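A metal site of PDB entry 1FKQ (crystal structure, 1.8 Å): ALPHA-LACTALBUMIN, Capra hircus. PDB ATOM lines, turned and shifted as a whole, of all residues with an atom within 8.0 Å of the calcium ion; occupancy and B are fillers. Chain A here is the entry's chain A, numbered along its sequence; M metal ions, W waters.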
ATOM      1  N   THR A  39     -25.986 -11.736 -25.568  1.00  0.00           N
ATOM      2  CA  THR A  39     -25.529 -13.106 -25.416  1.00  0.00           C
ATOM      3  C   THR A  39     -26.615 -14.166 -25.632  1.00  0.00           C
ATOM      4  O   THR A  39     -26.299 -15.338 -25.853  1.00  0.00           O
ATOM      5  CB  THR A  39     -24.905 -13.327 -24.031  1.00  0.00           C
ATOM      6  OG1 THR A  39     -25.878 -13.037 -23.026  1.00  0.00           O
ATOM      7  CG2 THR A  39     -23.698 -12.425 -23.841  1.00  0.00           C
ATOM      8  N   ILE A  76     -20.398 -29.212 -29.860  1.00  0.00           N
ATOM      9  CA  ILE A  76     -21.056 -28.640 -28.708  1.00  0.00           C
ATOM     10  C   ILE A  76     -22.530 -28.374 -28.979  1.00  0.00           C
ATOM     11  O   ILE A  76     -22.947 -28.242 -30.125  1.00  0.00           O
ATOM     12  CB  ILE A  76     -20.381 -27.293 -28.316  1.00  0.00           C
ATOM     13  CG1 ILE A  76     -20.852 -26.821 -26.936  1.00  0.00           C
ATOM     14  CG2 ILE A  76     -20.680 -26.226 -29.373  1.00  0.00           C
ATOM     15  CD1 ILE A  76     -20.038 -25.661 -26.394  1.00  0.00           C
ATOM     16  N   SER A  77     -23.297 -28.297 -27.899  1.00  0.00           N
ATOM     17  CA  SER A  77     -24.710 -28.008 -28.001  1.00  0.00           C
ATOM     18  C   SER A  77     -24.802 -26.504 -28.208  1.00  0.00           C
ATOM     19  O   SER A  77     -24.093 -25.738 -27.551  1.00  0.00           O
ATOM     20  CB  SER A  77     -25.410 -28.416 -26.699  1.00  0.00           C
ATOM     21  OG  SER A  77     -26.758 -27.985 -26.709  1.00  0.00           O
ATOM     22  N   CYS A  78     -25.660 -26.066 -29.132  1.00  0.00           N
ATOM     23  CA  CYS A  78     -25.815 -24.651 -29.418  1.00  0.00           C
ATOM     24  C   CYS A  78     -26.240 -23.834 -28.208  1.00  0.00           C
ATOM     25  O   CYS A  78     -25.846 -22.675 -28.046  1.00  0.00           O
ATOM     26  CB  CYS A  78     -26.843 -24.435 -30.525  1.00  0.00           C
ATOM     27  SG  CYS A  78     -26.413 -25.151 -32.133  1.00  0.00           S
ATOM     28  N   ASP A  79     -27.079 -24.435 -27.355  1.00  0.00           N
ATOM     29  CA  ASP A  79     -27.551 -23.728 -26.180  1.00  0.00           C
ATOM     30  C   ASP A  79     -26.401 -23.273 -25.280  1.00  0.00           C
ATOM     31  O   ASP A  79     -26.580 -22.430 -24.393  1.00  0.00           O
ATOM     32  CB  ASP A  79     -28.547 -24.613 -25.400  1.00  0.00           C
ATOM     33  CG  ASP A  79     -27.876 -25.774 -24.688  1.00  0.00           C
ATOM     34  OD1 ASP A  79     -28.473 -26.300 -23.722  1.00  0.00           O
ATOM     35  OD2 ASP A  79     -26.753 -26.163 -25.082  1.00  0.00           O
ATOM     36  N   LYS A  80     -25.214 -23.811 -25.509  1.00  0.00           N
ATOM     37  CA  LYS A  80     -24.036 -23.422 -24.731  1.00  0.00           C
ATOM     38  C   LYS A  80     -23.578 -22.026 -25.147  1.00  0.00           C
ATOM     39  O   LYS A  80     -22.747 -21.426 -24.474  1.00  0.00           O
ATOM     40  CB  LYS A  80     -22.904 -24.424 -24.955  1.00  0.00           C
ATOM     41  CG  LYS A  80     -22.956 -25.608 -24.028  1.00  0.00           C
ATOM     42  CD  LYS A  80     -22.864 -25.153 -22.586  1.00  0.00           C
ATOM     43  CE  LYS A  80     -23.575 -26.128 -21.668  1.00  0.00           C
ATOM     44  NZ  LYS A  80     -22.797 -27.375 -21.518  1.00  0.00           N
ATOM     45  N   PHE A  81     -24.131 -21.513 -26.249  1.00  0.00           N
ATOM     46  CA  PHE A  81     -23.775 -20.170 -26.720  1.00  0.00           C
ATOM     47  C   PHE A  81     -24.830 -19.150 -26.275  1.00  0.00           C
ATOM     48  O   PHE A  81     -24.839 -17.997 -26.734  1.00  0.00           O
ATOM     49  CB  PHE A  81     -23.661 -20.165 -28.245  1.00  0.00           C
ATOM     50  CG  PHE A  81     -22.614 -21.097 -28.773  1.00  0.00           C
ATOM     51  CD1 PHE A  81     -22.838 -21.798 -29.949  1.00  0.00           C
ATOM     52  CD2 PHE A  81     -21.398 -21.266 -28.106  1.00  0.00           C
ATOM     53  CE1 PHE A  81     -21.854 -22.663 -30.467  1.00  0.00           C
ATOM     54  CE2 PHE A  81     -20.408 -22.122 -28.616  1.00  0.00           C
ATOM     55  CZ  PHE A  81     -20.640 -22.818 -29.802  1.00  0.00           C
ATOM     56  N   LEU A  82     -25.715 -19.563 -25.379  1.00  0.00           N
ATOM     57  CA  LEU A  82     -26.765 -18.676 -24.915  1.00  0.00           C
ATOM     58  C   LEU A  82     -26.589 -18.214 -23.474  1.00  0.00           C
ATOM     59  O   LEU A  82     -27.407 -17.448 -22.959  1.00  0.00           O
ATOM     60  CB  LEU A  82     -28.134 -19.362 -25.088  1.00  0.00           C
ATOM     61  CG  LEU A  82     -28.551 -19.688 -26.522  1.00  0.00           C
ATOM     62  CD1 LEU A  82     -29.891 -20.389 -26.521  1.00  0.00           C
ATOM     63  CD2 LEU A  82     -28.613 -18.422 -27.352  1.00  0.00           C
ATOM     64  N   ASP A  83     -25.517 -18.658 -22.829  1.00  0.00           N
ATOM     65  CA  ASP A  83     -25.266 -18.240 -21.451  1.00  0.00           C
ATOM     66  C   ASP A  83     -24.305 -17.052 -21.356  1.00  0.00           C
ATOM     67  O   ASP A  83     -23.997 -16.407 -22.354  1.00  0.00           O
ATOM     68  CB  ASP A  83     -24.771 -19.419 -20.598  1.00  0.00           C
ATOM     69  CG  ASP A  83     -23.472 -20.006 -21.091  1.00  0.00           C
ATOM     70  OD1 ASP A  83     -22.628 -19.247 -21.603  1.00  0.00           O
ATOM     71  OD2 ASP A  83     -23.284 -21.246 -20.951  1.00  0.00           O
ATOM     72  N   ASP A  84     -23.849 -16.775 -20.137  1.00  0.00           N
ATOM     73  CA  ASP A  84     -22.969 -15.643 -19.883  1.00  0.00           C
ATOM     74  C   ASP A  84     -21.474 -15.907 -19.955  1.00  0.00           C
ATOM     75  O   ASP A  84     -20.674 -14.972 -19.917  1.00  0.00           O
ATOM     76  CB  ASP A  84     -23.288 -15.053 -18.527  1.00  0.00           C
ATOM     77  CG  ASP A  84     -23.763 -13.634 -18.627  1.00  0.00           C
ATOM     78  OD1 ASP A  84     -22.923 -12.745 -18.884  1.00  0.00           O
ATOM     79  OD2 ASP A  84     -24.978 -13.408 -18.454  1.00  0.00           O
ATOM     80  N   ASP A  85     -21.084 -17.176 -20.051  1.00  0.00           N
ATOM     81  CA  ASP A  85     -19.684 -17.557 -20.128  1.00  0.00           C
ATOM     82  C   ASP A  85     -19.258 -17.622 -21.598  1.00  0.00           C
ATOM     83  O   ASP A  85     -19.670 -18.525 -22.312  1.00  0.00           O
ATOM     84  CB  ASP A  85     -19.484 -18.921 -19.474  1.00  0.00           C
ATOM     85  CG  ASP A  85     -18.026 -19.241 -19.216  1.00  0.00           C
ATOM     86  OD1 ASP A  85     -17.161 -18.480 -19.677  1.00  0.00           O
ATOM     87  OD2 ASP A  85     -17.767 -20.260 -18.541  1.00  0.00           O
ATOM     88  N   LEU A  86     -18.445 -16.683 -22.035  1.00  0.00           N
ATOM     89  CA  LEU A  86     -18.028 -16.652 -23.428  1.00  0.00           C
ATOM     90  C   LEU A  86     -16.874 -17.588 -23.803  1.00  0.00           C
ATOM     91  O   LEU A  86     -16.459 -17.616 -24.965  1.00  0.00           O
ATOM     92  CB  LEU A  86     -17.666 -15.225 -23.820  1.00  0.00           C
ATOM     93  CG  LEU A  86     -18.753 -14.317 -24.420  1.00  0.00           C
ATOM     94  CD1 LEU A  86     -20.118 -14.980 -24.394  1.00  0.00           C
ATOM     95  CD2 LEU A  86     -18.764 -13.003 -23.669  1.00  0.00           C
ATOM     96  N   THR A  87     -16.361 -18.363 -22.855  1.00  0.00           N
ATOM     97  CA  THR A  87     -15.233 -19.253 -23.146  1.00  0.00           C
ATOM     98  C   THR A  87     -15.435 -20.269 -24.276  1.00  0.00           C
ATOM     99  O   THR A  87     -14.568 -20.413 -25.143  1.00  0.00           O
ATOM    100  CB  THR A  87     -14.774 -19.981 -21.883  1.00  0.00           C
ATOM    101  OG1 THR A  87     -14.706 -19.043 -20.805  1.00  0.00           O
ATOM    102  CG2 THR A  87     -13.389 -20.578 -22.102  1.00  0.00           C
ATOM    103  N   ASP A  88     -16.553 -20.986 -24.290  1.00  0.00           N
ATOM    104  CA  ASP A  88     -16.767 -21.945 -25.367  1.00  0.00           C
ATOM    105  C   ASP A  88     -17.148 -21.221 -26.659  1.00  0.00           C
ATOM    106  O   ASP A  88     -16.813 -21.685 -27.749  1.00  0.00           O
ATOM    107  CB  ASP A  88     -17.834 -22.983 -25.001  1.00  0.00           C
ATOM    108  CG  ASP A  88     -18.983 -22.403 -24.211  1.00  0.00           C
ATOM    109  OD1 ASP A  88     -19.253 -21.200 -24.347  1.00  0.00           O
ATOM    110  OD2 ASP A  88     -19.607 -23.169 -23.443  1.00  0.00           O
ATOM    111  N   ASP A  89     -17.831 -20.086 -26.549  1.00  0.00           N
ATOM    112  CA  ASP A  89     -18.195 -19.309 -27.736  1.00  0.00           C
ATOM    113  C   ASP A  89     -16.921 -18.953 -28.487  1.00  0.00           C
ATOM    114  O   ASP A  89     -16.828 -19.114 -29.705  1.00  0.00           O
ATOM    115  CB  ASP A  89     -18.909 -17.994 -27.359  1.00  0.00           C
ATOM    116  CG  ASP A  89     -20.188 -18.210 -26.578  1.00  0.00           C
ATOM    117  OD1 ASP A  89     -21.271 -17.802 -27.066  1.00  0.00           O
ATOM    118  OD2 ASP A  89     -20.115 -18.767 -25.467  1.00  0.00           O
ATOM    119  N   ILE A  90     -15.939 -18.457 -27.736  1.00  0.00           N
ATOM    120  CA  ILE A  90     -14.643 -18.040 -28.274  1.00  0.00           C
ATOM    121  C   ILE A  90     -13.867 -19.181 -28.927  1.00  0.00           C
ATOM    122  O   ILE A  90     -13.232 -18.983 -29.957  1.00  0.00           O
ATOM    123  CB  ILE A  90     -13.790 -17.375 -27.165  1.00  0.00           C
ATOM    124  CG1 ILE A  90     -14.334 -15.977 -26.868  1.00  0.00           C
ATOM    125  CG2 ILE A  90     -12.338 -17.257 -27.596  1.00  0.00           C
ATOM    126  CD1 ILE A  90     -13.884 -15.403 -25.530  1.00  0.00           C
HETATM  127 CA    CA M   1     -21.066 -19.906 -23.548  1.00  0.00          CA
HETATM  128  O   HOH W   1     -20.668 -21.720 -21.766  1.00  0.00           O
HETATM  129  O   HOH W   2     -22.613 -17.967 -24.212  1.00  0.00           O
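The calcium ion is bound by the backbone carbonyl oxygen of Asp 85 (2.3 Å), the side-chain carboxylate of Asp 88 (2.4 Å), the side-chain carboxylate of Asp 89 (2.4 Å), the backbone carbonyl oxygen of Lys 80 (2.4 Å), water W2 (2.6 Å), water W1 (2.6 Å) and the side-chain carboxylate of Asp 83 (2.6 Å). The calcium ion has seven donor atoms within binding distance.
Within 4 Å of the calcium ion: Lys 80, Asp 83, Asp 85, Asp 88 and Asp 89. The nearest printed residue that does not touch the calcium ion is Phe 81 (4.2 Å).
Water W1 lies within hydrogen-bond range of OD2 of Asp 88 (2.5 Å) and OD2 of Asp 83 (2.8 Å).
OD1 of Asp 85 sits at hydrogen-bond distance from OG1 of Thr 87 (2.8 Å).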
